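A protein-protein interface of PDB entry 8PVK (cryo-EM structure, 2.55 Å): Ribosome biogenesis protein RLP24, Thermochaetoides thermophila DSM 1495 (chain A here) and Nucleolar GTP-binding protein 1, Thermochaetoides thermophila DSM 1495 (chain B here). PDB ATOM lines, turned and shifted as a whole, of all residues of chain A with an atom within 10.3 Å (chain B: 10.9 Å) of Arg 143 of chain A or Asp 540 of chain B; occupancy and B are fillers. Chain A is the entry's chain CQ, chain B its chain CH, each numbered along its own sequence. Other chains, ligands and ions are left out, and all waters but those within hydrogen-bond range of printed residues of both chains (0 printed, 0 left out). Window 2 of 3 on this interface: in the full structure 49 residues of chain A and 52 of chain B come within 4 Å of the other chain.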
ATOM      1  N   LEU A 137      17.774  27.554 -15.612  1.00  0.00           N
ATOM      2  CA  LEU A 137      16.363  27.831 -15.398  1.00  0.00           C
ATOM      3  C   LEU A 137      16.044  27.907 -13.910  1.00  0.00           C
ATOM      4  O   LEU A 137      16.723  27.306 -13.073  1.00  0.00           O
ATOM      5  CB  LEU A 137      15.484  26.756 -16.041  1.00  0.00           C
ATOM      6  CG  LEU A 137      15.105  26.796 -17.524  1.00  0.00           C
ATOM      7  CD1 LEU A 137      14.279  28.034 -17.825  1.00  0.00           C
ATOM      8  CD2 LEU A 137      16.305  26.692 -18.447  1.00  0.00           C
ATOM      9  N   ARG A 138      14.995  28.658 -13.590  1.00  0.00           N
ATOM     10  CA  ARG A 138      14.450  28.634 -12.244  1.00  0.00           C
ATOM     11  C   ARG A 138      13.618  27.373 -12.036  1.00  0.00           C
ATOM     12  O   ARG A 138      13.234  26.689 -12.987  1.00  0.00           O
ATOM     13  CB  ARG A 138      13.596  29.876 -11.985  1.00  0.00           C
ATOM     14  CG  ARG A 138      14.394  31.138 -11.703  1.00  0.00           C
ATOM     15  CD  ARG A 138      13.514  32.374 -11.794  1.00  0.00           C
ATOM     16  NE  ARG A 138      14.096  33.516 -11.100  1.00  0.00           N
ATOM     17  CZ  ARG A 138      13.817  33.853  -9.848  1.00  0.00           C
ATOM     18  NH1 ARG A 138      12.964  33.153  -9.118  1.00  0.00           N
ATOM     19  NH2 ARG A 138      14.406  34.919  -9.316  1.00  0.00           N
ATOM     20  N   GLY A 139      13.352  27.057 -10.767  1.00  0.00           N
ATOM     21  CA  GLY A 139      12.503  25.915 -10.464  1.00  0.00           C
ATOM     22  C   GLY A 139      11.068  26.118 -10.912  1.00  0.00           C
ATOM     23  O   GLY A 139      10.452  25.214 -11.486  1.00  0.00           O
ATOM     24  N   SER A 140      10.520  27.312 -10.666  1.00  0.00           N
ATOM     25  CA  SER A 140       9.173  27.628 -11.133  1.00  0.00           C
ATOM     26  C   SER A 140       9.114  27.673 -12.655  1.00  0.00           C
ATOM     27  O   SER A 140       8.116  27.256 -13.255  1.00  0.00           O
ATOM     28  CB  SER A 140       8.710  28.956 -10.536  1.00  0.00           C
ATOM     29  OG  SER A 140       9.615  29.999 -10.850  1.00  0.00           O
ATOM     30  N   GLU A 141      10.175  28.178 -13.294  1.00  0.00           N
ATOM     31  CA  GLU A 141      10.237  28.178 -14.753  1.00  0.00           C
ATOM     32  C   GLU A 141      10.280  26.760 -15.306  1.00  0.00           C
ATOM     33  O   GLU A 141       9.616  26.464 -16.305  1.00  0.00           O
ATOM     34  CB  GLU A 141      11.451  28.978 -15.228  1.00  0.00           C
ATOM     35  CG  GLU A 141      11.342  30.474 -14.982  1.00  0.00           C
ATOM     36  CD  GLU A 141      12.654  31.199 -15.216  1.00  0.00           C
ATOM     37  OE1 GLU A 141      13.694  30.522 -15.355  1.00  0.00           O
ATOM     38  OE2 GLU A 141      12.644  32.447 -15.261  1.00  0.00           O
ATOM     39  N   LYS A 142      11.046  25.871 -14.665  1.00  0.00           N
ATOM     40  CA  LYS A 142      11.076  24.471 -15.080  1.00  0.00           C
ATOM     41  C   LYS A 142       9.714  23.813 -14.908  1.00  0.00           C
ATOM     42  O   LYS A 142       9.274  23.051 -15.775  1.00  0.00           O
ATOM     43  CB  LYS A 142      12.133  23.702 -14.287  1.00  0.00           C
ATOM     44  CG  LYS A 142      13.560  23.914 -14.752  1.00  0.00           C
ATOM     45  CD  LYS A 142      14.494  22.898 -14.112  1.00  0.00           C
ATOM     46  CE  LYS A 142      15.945  23.149 -14.492  1.00  0.00           C
ATOM     47  NZ  LYS A 142      16.490  24.372 -13.844  1.00  0.00           N
ATOM     48  N   ARG A 143       9.030  24.105 -13.796  1.00  0.00           N
ATOM     49  CA  ARG A 143       7.701  23.547 -13.558  1.00  0.00           C
ATOM     50  C   ARG A 143       6.702  24.019 -14.611  1.00  0.00           C
ATOM     51  O   ARG A 143       5.939  23.217 -15.167  1.00  0.00           O
ATOM     52  CB  ARG A 143       7.223  23.928 -12.156  1.00  0.00           C
ATOM     53  CG  ARG A 143       6.132  23.033 -11.594  1.00  0.00           C
ATOM     54  CD  ARG A 143       6.718  21.857 -10.834  1.00  0.00           C
ATOM     55  NE  ARG A 143       5.756  21.282  -9.901  1.00  0.00           N
ATOM     56  CZ  ARG A 143       6.052  20.366  -8.988  1.00  0.00           C
ATOM     57  NH1 ARG A 143       7.281  19.894  -8.857  1.00  0.00           N
ATOM     58  NH2 ARG A 143       5.092  19.914  -8.187  1.00  0.00           N
ATOM     59  N   ARG A 144       6.707  25.321 -14.912  1.00  0.00           N
ATOM     60  CA  ARG A 144       5.748  25.848 -15.876  1.00  0.00           C
ATOM     61  C   ARG A 144       6.074  25.402 -17.298  1.00  0.00           C
ATOM     62  O   ARG A 144       5.155  25.142 -18.083  1.00  0.00           O
ATOM     63  CB  ARG A 144       5.657  27.377 -15.762  1.00  0.00           C
ATOM     64  CG  ARG A 144       6.715  28.186 -16.500  1.00  0.00           C
ATOM     65  CD  ARG A 144       6.151  29.518 -16.966  1.00  0.00           C
ATOM     66  NE  ARG A 144       7.027  30.177 -17.927  1.00  0.00           N
ATOM     67  CZ  ARG A 144       6.730  31.303 -18.559  1.00  0.00           C
ATOM     68  NH1 ARG A 144       5.582  31.929 -18.355  1.00  0.00           N
ATOM     69  NH2 ARG A 144       7.607  31.817 -19.418  1.00  0.00           N
ATOM     70  N   LEU A 145       7.358  25.241 -17.636  1.00  0.00           N
ATOM     71  CA  LEU A 145       7.698  24.736 -18.960  1.00  0.00           C
ATOM     72  C   LEU A 145       7.370  23.257 -19.093  1.00  0.00           C
ATOM     73  O   LEU A 145       6.935  22.819 -20.163  1.00  0.00           O
ATOM     74  CB  LEU A 145       9.174  24.992 -19.264  1.00  0.00           C
ATOM     75  CG  LEU A 145       9.552  26.441 -19.585  1.00  0.00           C
ATOM     76  CD1 LEU A 145      10.965  26.517 -20.135  1.00  0.00           C
ATOM     77  CD2 LEU A 145       8.563  27.070 -20.556  1.00  0.00           C
ATOM     78  N   ALA A 146       7.542  22.482 -18.016  1.00  0.00           N
ATOM     79  CA  ALA A 146       7.154  21.076 -18.042  1.00  0.00           C
ATOM     80  C   ALA A 146       5.649  20.917 -18.203  1.00  0.00           C
ATOM     81  O   ALA A 146       5.191  20.080 -18.991  1.00  0.00           O
ATOM     82  CB  ALA A 146       7.636  20.376 -16.771  1.00  0.00           C
ATOM     83  N   GLU A 147       4.857  21.725 -17.489  1.00  0.00           N
ATOM     84  CA  GLU A 147       3.408  21.597 -17.629  1.00  0.00           C
ATOM     85  C   GLU A 147       2.922  22.128 -18.977  1.00  0.00           C
ATOM     86  O   GLU A 147       1.975  21.573 -19.547  1.00  0.00           O
ATOM     87  CB  GLU A 147       2.683  22.277 -16.459  1.00  0.00           C
ATOM     88  CG  GLU A 147       2.731  23.794 -16.415  1.00  0.00           C
ATOM     89  CD  GLU A 147       1.506  24.437 -17.036  1.00  0.00           C
ATOM     90  OE1 GLU A 147       0.470  23.750 -17.160  1.00  0.00           O
ATOM     91  OE2 GLU A 147       1.579  25.629 -17.401  1.00  0.00           O
ATOM     92  N   LEU A 148       3.573  23.164 -19.524  1.00  0.00           N
ATOM     93  CA  LEU A 148       3.215  23.632 -20.861  1.00  0.00           C
ATOM     94  C   LEU A 148       3.567  22.601 -21.926  1.00  0.00           C
ATOM     95  O   LEU A 148       2.805  22.404 -22.880  1.00  0.00           O
ATOM     96  CB  LEU A 148       3.900  24.966 -21.155  1.00  0.00           C
ATOM     97  CG  LEU A 148       3.233  26.212 -20.571  1.00  0.00           C
ATOM     98  CD1 LEU A 148       4.137  27.425 -20.720  1.00  0.00           C
ATOM     99  CD2 LEU A 148       1.885  26.458 -21.230  1.00  0.00           C
ATOM    100  N   ALA A 149       4.716  21.933 -21.781  1.00  0.00           N
ATOM    101  CA  ALA A 149       5.089  20.881 -22.720  1.00  0.00           C
ATOM    102  C   ALA A 149       4.151  19.686 -22.615  1.00  0.00           C
ATOM    103  O   ALA A 149       3.807  19.071 -23.630  1.00  0.00           O
ATOM    104  CB  ALA A 149       6.537  20.452 -22.481  1.00  0.00           C
ATOM    105  N   ALA A 150       3.724  19.345 -21.395  1.00  0.00           N
ATOM    106  CA  ALA A 150       2.765  18.258 -21.222  1.00  0.00           C
ATOM    107  C   ALA A 150       1.406  18.614 -21.815  1.00  0.00           C
ATOM    108  O   ALA A 150       0.719  17.747 -22.368  1.00  0.00           O
ATOM    109  CB  ALA A 150       2.630  17.910 -19.740  1.00  0.00           C
ATOM    110  N   GLU A 151       1.001  19.882 -21.708  1.00  0.00           N
ATOM    111  CA  GLU A 151      -0.287  20.293 -22.259  1.00  0.00           C
ATOM    112  C   GLU A 151      -0.256  20.353 -23.782  1.00  0.00           C
ATOM    113  O   GLU A 151      -1.198  19.902 -24.443  1.00  0.00           O
ATOM    114  CB  GLU A 151      -0.696  21.645 -21.677  1.00  0.00           C
ATOM    115  N   VAL A 156      10.201  19.540 -24.002  1.00  0.00           N
ATOM    116  CA  VAL A 156      10.590  20.307 -22.823  1.00  0.00           C
ATOM    117  C   VAL A 156      11.974  20.908 -23.005  1.00  0.00           C
ATOM    118  O   VAL A 156      12.234  22.029 -22.554  1.00  0.00           O
ATOM    119  CB  VAL A 156      10.522  19.422 -21.562  1.00  0.00           C
ATOM    120  N   LEU A 159      11.410  24.075 -25.244  1.00  0.00           N
ATOM    121  CA  LEU A 159      10.959  25.224 -24.457  1.00  0.00           C
ATOM    122  C   LEU A 159      12.038  25.717 -23.500  1.00  0.00           C
ATOM    123  O   LEU A 159      12.158  26.929 -23.279  1.00  0.00           O
ATOM    124  CB  LEU A 159       9.672  24.904 -23.688  1.00  0.00           C
ATOM    125  CG  LEU A 159       8.312  24.902 -24.406  1.00  0.00           C
ATOM    126  CD1 LEU A 159       8.098  23.736 -25.353  1.00  0.00           C
ATOM    127  CD2 LEU A 159       7.181  24.967 -23.384  1.00  0.00           C
ATOM    128  N   GLU A 160      12.846  24.805 -22.945  1.00  0.00           N
ATOM    129  CA  GLU A 160      13.928  25.206 -22.053  1.00  0.00           C
ATOM    130  C   GLU A 160      14.983  26.030 -22.780  1.00  0.00           C
ATOM    131  O   GLU A 160      15.435  27.057 -22.262  1.00  0.00           O
ATOM    132  CB  GLU A 160      14.562  23.972 -21.412  1.00  0.00           C
ATOM    133  CG  GLU A 160      13.985  23.613 -20.051  1.00  0.00           C
ATOM    134  CD  GLU A 160      14.714  22.455 -19.395  1.00  0.00           C
ATOM    135  OE1 GLU A 160      15.280  21.616 -20.126  1.00  0.00           O
ATOM    136  OE2 GLU A 160      14.721  22.384 -18.147  1.00  0.00           O
ATOM    137  N   GLU A 163      13.518  29.482 -23.653  1.00  0.00           N
ATOM    138  CA  GLU A 163      13.507  30.353 -22.483  1.00  0.00           C
ATOM    139  C   GLU A 163      14.919  30.769 -22.085  1.00  0.00           C
ATOM    140  O   GLU A 163      15.118  31.891 -21.604  1.00  0.00           O
ATOM    141  CB  GLU A 163      12.791  29.656 -21.322  1.00  0.00           C
ATOM    142  CG  GLU A 163      12.667  30.486 -20.045  1.00  0.00           C
ATOM    143  CD  GLU A 163      11.791  31.716 -20.211  1.00  0.00           C
ATOM    144  OE1 GLU A 163      10.901  31.715 -21.089  1.00  0.00           O
ATOM    145  OE2 GLU A 163      11.991  32.691 -19.457  1.00  0.00           O
ATOM    146  N   LEU B 530      14.606  32.986   1.090  1.00  0.00           N
ATOM    147  CA  LEU B 530      15.135  31.633   0.919  1.00  0.00           C
ATOM    148  C   LEU B 530      14.556  30.958  -0.321  1.00  0.00           C
ATOM    149  O   LEU B 530      15.291  30.322  -1.090  1.00  0.00           O
ATOM    150  CB  LEU B 530      14.852  30.793   2.164  1.00  0.00           C
ATOM    151  CG  LEU B 530      15.335  29.341   2.111  1.00  0.00           C
ATOM    152  CD1 LEU B 530      16.821  29.260   1.789  1.00  0.00           C
ATOM    153  CD2 LEU B 530      15.030  28.628   3.412  1.00  0.00           C
ATOM    154  N   GLU B 531      13.243  31.092  -0.538  1.00  0.00           N
ATOM    155  CA  GLU B 531      12.620  30.515  -1.725  1.00  0.00           C
ATOM    156  C   GLU B 531      13.121  31.181  -2.998  1.00  0.00           C
ATOM    157  O   GLU B 531      13.327  30.503  -4.009  1.00  0.00           O
ATOM    158  CB  GLU B 531      11.097  30.613  -1.638  1.00  0.00           C
ATOM    159  CG  GLU B 531      10.472  29.756  -0.552  1.00  0.00           C
ATOM    160  CD  GLU B 531       8.964  29.904  -0.495  1.00  0.00           C
ATOM    161  OE1 GLU B 531       8.423  30.766  -1.218  1.00  0.00           O
ATOM    162  OE2 GLU B 531       8.321  29.157   0.271  1.00  0.00           O
ATOM    163  N   ASP B 532      13.328  32.501  -2.970  1.00  0.00           N
ATOM    164  CA  ASP B 532      13.851  33.195  -4.144  1.00  0.00           C
ATOM    165  C   ASP B 532      15.269  32.741  -4.472  1.00  0.00           C
ATOM    166  O   ASP B 532      15.597  32.515  -5.643  1.00  0.00           O
ATOM    167  CB  ASP B 532      13.810  34.706  -3.920  1.00  0.00           C
ATOM    168  CG  ASP B 532      14.099  35.490  -5.184  1.00  0.00           C
ATOM    169  OD1 ASP B 532      13.929  34.930  -6.287  1.00  0.00           O
ATOM    170  OD2 ASP B 532      14.495  36.670  -5.075  1.00  0.00           O
ATOM    171  N   HIS B 533      16.118  32.585  -3.450  1.00  0.00           N
ATOM    172  CA  HIS B 533      17.487  32.140  -3.696  1.00  0.00           C
ATOM    173  C   HIS B 533      17.528  30.699  -4.195  1.00  0.00           C
ATOM    174  O   HIS B 533      18.299  30.379  -5.107  1.00  0.00           O
ATOM    175  CB  HIS B 533      18.332  32.289  -2.433  1.00  0.00           C
ATOM    176  CG  HIS B 533      19.776  31.954  -2.637  1.00  0.00           C
ATOM    177  ND1 HIS B 533      20.676  32.845  -3.183  1.00  0.00           N
ATOM    178  CD2 HIS B 533      20.473  30.821  -2.389  1.00  0.00           C
ATOM    179  CE1 HIS B 533      21.867  32.279  -3.251  1.00  0.00           C
ATOM    180  NE2 HIS B 533      21.771  31.050  -2.774  1.00  0.00           N
ATOM    181  N   LEU B 534      16.704  29.819  -3.618  1.00  0.00           N
ATOM    182  CA  LEU B 534      16.678  28.434  -4.082  1.00  0.00           C
ATOM    183  C   LEU B 534      16.086  28.319  -5.482  1.00  0.00           C
ATOM    184  O   LEU B 534      16.531  27.480  -6.275  1.00  0.00           O
ATOM    185  CB  LEU B 534      15.901  27.563  -3.097  1.00  0.00           C
ATOM    186  CG  LEU B 534      16.616  27.267  -1.777  1.00  0.00           C
ATOM    187  CD1 LEU B 534      15.784  26.338  -0.912  1.00  0.00           C
ATOM    188  CD2 LEU B 534      17.997  26.677  -2.030  1.00  0.00           C
ATOM    189  N   ASP B 535      15.093  29.153  -5.804  1.00  0.00           N
ATOM    190  CA  ASP B 535      14.541  29.184  -7.152  1.00  0.00           C
ATOM    191  C   ASP B 535      15.572  29.677  -8.159  1.00  0.00           C
ATOM    192  O   ASP B 535      15.660  29.145  -9.270  1.00  0.00           O
ATOM    193  CB  ASP B 535      13.292  30.066  -7.172  1.00  0.00           C
ATOM    194  CG  ASP B 535      12.432  29.837  -8.396  1.00  0.00           C
ATOM    195  OD1 ASP B 535      11.964  28.695  -8.592  1.00  0.00           O
ATOM    196  OD2 ASP B 535      12.210  30.803  -9.153  1.00  0.00           O
ATOM    197  N   GLN B 536      16.358  30.691  -7.787  1.00  0.00           N
ATOM    198  CA  GLN B 536      17.424  31.165  -8.666  1.00  0.00           C
ATOM    199  C   GLN B 536      18.502  30.104  -8.851  1.00  0.00           C
ATOM    200  O   GLN B 536      19.033  29.936  -9.955  1.00  0.00           O
ATOM    201  CB  GLN B 536      18.021  32.458  -8.111  1.00  0.00           C
ATOM    202  CG  GLN B 536      19.080  33.087  -8.998  1.00  0.00           C
ATOM    203  CD  GLN B 536      19.603  34.395  -8.441  1.00  0.00           C
ATOM    204  OE1 GLN B 536      19.200  34.828  -7.362  1.00  0.00           O
ATOM    205  NE2 GLN B 536      20.505  35.034  -9.178  1.00  0.00           N
ATOM    206  N   LEU B 537      18.834  29.370  -7.786  1.00  0.00           N
ATOM    207  CA  LEU B 537      19.786  28.271  -7.899  1.00  0.00           C
ATOM    208  C   LEU B 537      19.225  27.078  -8.663  1.00  0.00           C
ATOM    209  O   LEU B 537      20.008  26.244  -9.131  1.00  0.00           O
ATOM    210  CB  LEU B 537      20.241  27.818  -6.511  1.00  0.00           C
ATOM    211  CG  LEU B 537      21.235  28.721  -5.780  1.00  0.00           C
ATOM    212  CD1 LEU B 537      21.746  28.037  -4.524  1.00  0.00           C
ATOM    213  CD2 LEU B 537      22.391  29.103  -6.690  1.00  0.00           C
ATOM    214  N   GLY B 538      17.909  26.972  -8.795  1.00  0.00           N
ATOM    215  CA  GLY B 538      17.298  25.918  -9.570  1.00  0.00           C
ATOM    216  C   GLY B 538      16.682  24.791  -8.776  1.00  0.00           C
ATOM    217  O   GLY B 538      16.715  23.645  -9.237  1.00  0.00           O
ATOM    218  N   VAL B 539      16.122  25.074  -7.604  1.00  0.00           N
ATOM    219  CA  VAL B 539      15.522  24.065  -6.740  1.00  0.00           C
ATOM    220  C   VAL B 539      14.030  24.346  -6.642  1.00  0.00           C
ATOM    221  O   VAL B 539      13.623  25.477  -6.350  1.00  0.00           O
ATOM    222  CB  VAL B 539      16.175  24.059  -5.347  1.00  0.00           C
ATOM    223  CG1 VAL B 539      15.558  22.980  -4.472  1.00  0.00           C
ATOM    224  CG2 VAL B 539      17.678  23.862  -5.468  1.00  0.00           C
ATOM    225  N   ASP B 540      13.217  23.322  -6.891  1.00  0.00           N
ATOM    226  CA  ASP B 540      11.767  23.454  -6.810  1.00  0.00           C
ATOM    227  C   ASP B 540      11.362  23.522  -5.343  1.00  0.00           C
ATOM    228  O   ASP B 540      11.468  22.528  -4.617  1.00  0.00           O
ATOM    229  CB  ASP B 540      11.084  22.290  -7.521  1.00  0.00           C
ATOM    230  CG  ASP B 540       9.605  22.532  -7.748  1.00  0.00           C
ATOM    231  OD1 ASP B 540       8.818  22.375  -6.790  1.00  0.00           O
ATOM    232  OD2 ASP B 540       9.229  22.882  -8.885  1.00  0.00           O
ATOM    233  N   THR B 541      10.901  24.695  -4.906  1.00  0.00           N
ATOM    234  CA  THR B 541      10.539  24.873  -3.503  1.00  0.00           C
ATOM    235  C   THR B 541       9.220  24.191  -3.166  1.00  0.00           C
ATOM    236  O   THR B 541       9.014  23.779  -2.018  1.00  0.00           O
ATOM    237  CB  THR B 541      10.463  26.360  -3.164  1.00  0.00           C
ATOM    238  OG1 THR B 541       9.350  26.951  -3.845  1.00  0.00           O
ATOM    239  CG2 THR B 541      11.741  27.067  -3.591  1.00  0.00           C
ATOM    240  N   GLU B 542       8.316  24.070  -4.141  1.00  0.00           N
ATOM    241  CA  GLU B 542       7.038  23.415  -3.888  1.00  0.00           C
ATOM    242  C   GLU B 542       7.201  21.913  -3.699  1.00  0.00           C
ATOM    243  O   GLU B 542       6.424  21.295  -2.963  1.00  0.00           O
ATOM    244  CB  GLU B 542       6.063  23.705  -5.029  1.00  0.00           C
ATOM    245  CG  GLU B 542       5.565  25.142  -5.072  1.00  0.00           C
ATOM    246  CD  GLU B 542       6.418  26.032  -5.955  1.00  0.00           C
ATOM    247  OE1 GLU B 542       7.634  26.147  -5.693  1.00  0.00           O
ATOM    248  OE2 GLU B 542       5.871  26.619  -6.913  1.00  0.00           O
ATOM    249  N   ALA B 543       8.199  21.310  -4.348  1.00  0.00           N
ATOM    250  CA  ALA B 543       8.426  19.877  -4.212  1.00  0.00           C
ATOM    251  C   ALA B 543       9.060  19.502  -2.880  1.00  0.00           C
ATOM    252  O   ALA B 543       9.046  18.322  -2.515  1.00  0.00           O
ATOM    253  CB  ALA B 543       9.302  19.370  -5.358  1.00  0.00           C
ATOM    254  N   ILE B 544       9.613  20.467  -2.151  1.00  0.00           N
ATOM    255  CA  ILE B 544      10.230  20.198  -0.860  1.00  0.00           C
ATOM    256  C   ILE B 544       9.452  20.796   0.308  1.00  0.00           C
ATOM    257  O   ILE B 544       9.628  20.332   1.446  1.00  0.00           O
ATOM    258  CB  ILE B 544      11.696  20.677  -0.828  1.00  0.00           C
ATOM    259  CG1 ILE B 544      11.772  22.189  -1.034  1.00  0.00           C
ATOM    260  CG2 ILE B 544      12.520  19.946  -1.876  1.00  0.00           C
ATOM    261  CD1 ILE B 544      13.144  22.763  -0.788  1.00  0.00           C
ATOM    262  N   GLY B 545       8.602  21.796   0.075  1.00  0.00           N
ATOM    263  CA  GLY B 545       7.736  22.311   1.118  1.00  0.00           C
ATOM    264  C   GLY B 545       8.433  23.088   2.216  1.00  0.00           C
ATOM    265  O   GLY B 545       8.491  22.634   3.363  1.00  0.00           O
ATOM    266  N   LEU B 546       8.967  24.263   1.880  1.00  0.00           N
ATOM    267  CA  LEU B 546       9.610  25.111   2.876  1.00  0.00           C
ATOM    268  C   LEU B 546       8.614  25.818   3.786  1.00  0.00           C
ATOM    269  O   LEU B 546       9.017  26.348   4.829  1.00  0.00           O
ATOM    270  CB  LEU B 546      10.497  26.150   2.188  1.00  0.00           C
ATOM    271  CG  LEU B 546      11.683  25.618   1.384  1.00  0.00           C
ATOM    272  CD1 LEU B 546      12.420  26.765   0.717  1.00  0.00           C
ATOM    273  CD2 LEU B 546      12.620  24.827   2.280  1.00  0.00           C
ATOM    274  N   ARG B 547       7.330  25.843   3.411  1.00  0.00           N
ATOM    275  CA  ARG B 547       6.319  26.501   4.233  1.00  0.00           C
ATOM    276  C   ARG B 547       6.139  25.790   5.569  1.00  0.00           C
ATOM    277  O   ARG B 547       5.958  26.438   6.606  1.00  0.00           O
ATOM    278  CB  ARG B 547       4.990  26.562   3.479  1.00  0.00           C
ATOM    279  CG  ARG B 547       5.126  26.888   2.000  1.00  0.00           C
ATOM    280  CD  ARG B 547       5.468  28.351   1.784  1.00  0.00           C
ATOM    281  NE  ARG B 547       4.467  29.242   2.358  1.00  0.00           N
ATOM    282  CZ  ARG B 547       4.445  30.556   2.180  1.00  0.00           C
ATOM    283  NH1 ARG B 547       5.358  31.169   1.446  1.00  0.00           N
ATOM    284  NH2 ARG B 547       3.482  31.272   2.754  1.00  0.00           N
ATOM    285  N   ARG B 549       8.502  23.994   7.017  1.00  0.00           N
ATOM    286  CA  ARG B 549       9.745  24.146   7.765  1.00  0.00           C
ATOM    287  C   ARG B 549       9.878  25.541   8.361  1.00  0.00           C
ATOM    288  O   ARG B 549      10.547  25.713   9.387  1.00  0.00           O
ATOM    289  CB  ARG B 549      10.937  23.841   6.861  1.00  0.00           C
ATOM    290  CG  ARG B 549      10.919  22.442   6.278  1.00  0.00           C
ATOM    291  CD  ARG B 549      11.972  22.287   5.201  1.00  0.00           C
ATOM    292  NE  ARG B 549      11.824  21.032   4.475  1.00  0.00           N
ATOM    293  CZ  ARG B 549      12.515  20.711   3.390  1.00  0.00           C
ATOM    294  NH1 ARG B 549      13.422  21.530   2.882  1.00  0.00           N
ATOM    295  NH2 ARG B 549      12.291  19.541   2.800  1.00  0.00           N
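Of the 19 printed residues of chain B, 4 touch a printed residue of chain A.
Of the 19 printed residues of chain A, 5 touch a printed residue of chain B.
Among the printed residues, 7 pairs touch across the chains.
Among the printed residues, Asp or Glu carboxylates within 4 Å of a Lys or Arg side-chain nitrogen of the other chain: Arg 138 of chain A with Asp 532 of chain B (3.1 Å), Arg 138 of chain A with Asp 535 of chain B (2.5 Å) and Arg 143 of chain A with Asp 540 of chain B (3.6 Å).
Leu 137 of chain A touches Gly 538 of chain B (O to CA, 3.8 Å).
Gly 139 of chain A touches Asp 540 of chain B.
Of chain A, only Gly 139 and Arg 143 come within 4 Å of Asp 540 of chain B.
Of chain B, only Asp 535 and Asp 540 come within 4 Å of Gly 139 of chain A.
Ser 140 of chain A touches one residue of chain B.
Gly 538 of chain B touches just one residue of chain A: Leu 137 (3.8 Å).
Val 539 of chain B touches none of the printed residues of chain A.
No residue of chain A comes within 4 Å of Thr 541 of chain B.
No residue of chain A comes within 4 Å of Glu 542 of chain B.
No residue of chain A comes within 4 Å of Ala 543 of chain B.
Of the printed residues of chain A, Asp 532 of chain B touches Arg 138 (3.1 Å).
Of the printed residues of chain B, Leu 137 of chain A touches Gly 538.
Printed residues of chain A within 4 Å of Asp 535 of chain B: Arg 138 (2.5 Å), Gly 139 (3.1 Å) and Ser 140 (2.9 Å).
Glu 160 of chain A touches none of the printed residues of chain B.
Glu 163 of chain A touches none of the printed residues of chain B.
The nearest residue of chain A that does not touch Asp 540 of chain B is Ser 140 of chain A (4.9 Å).
The nearest printed residue of chain A that does not touch Asp 532 of chain B is Gly 139 of chain A (7.8 Å).
The side-chain carboxylate of Asp 535 of chain B lies within hydrogen-bond range of the backbone NH of Gly 139 of chain A (3.1 Å).
OD1 of Asp 532 of chain B is in salt-bridge range of NH2 of Arg 138 of chain A (3.1 Å).
The side-chain carboxylate (OD2) of Asp 540 of chain B lies within salt-bridge range of the guanidinium group (NH1) of Arg 143 of chain A (3.6 Å).
The side-chain carboxylate (OD1) of Asp 535 of chain B lies within hydrogen-bond range of the backbone NH (N) of Ser 140 of chain A, at 2.9 Å.
The side-chain carboxylate (OD2) of Asp 535 of chain B lies within salt-bridge range of the guanidinium group (NH1) of Arg 138 of chain A (2.5 Å).
The side-chain carboxylate of Asp 540 of chain B lies within hydrogen-bond range of the backbone NH of Glu 542 of chain B (3.2 Å).
The side-chain amino group of Lys 142 of chain A sits at hydrogen-bond distance from the backbone carbonyl oxygen of Leu 137 of chain A, at 3.0 Å.
The side-chain carboxylate (OE1) of Glu 141 of chain A is in hydrogen-bond range of the backbone NH (N) of Arg 138 of chain A, 2.9 Å away.
The side-chain carboxylate of Asp 540 of chain B lies within hydrogen-bond range of the backbone NH of Ala 543 of chain B.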
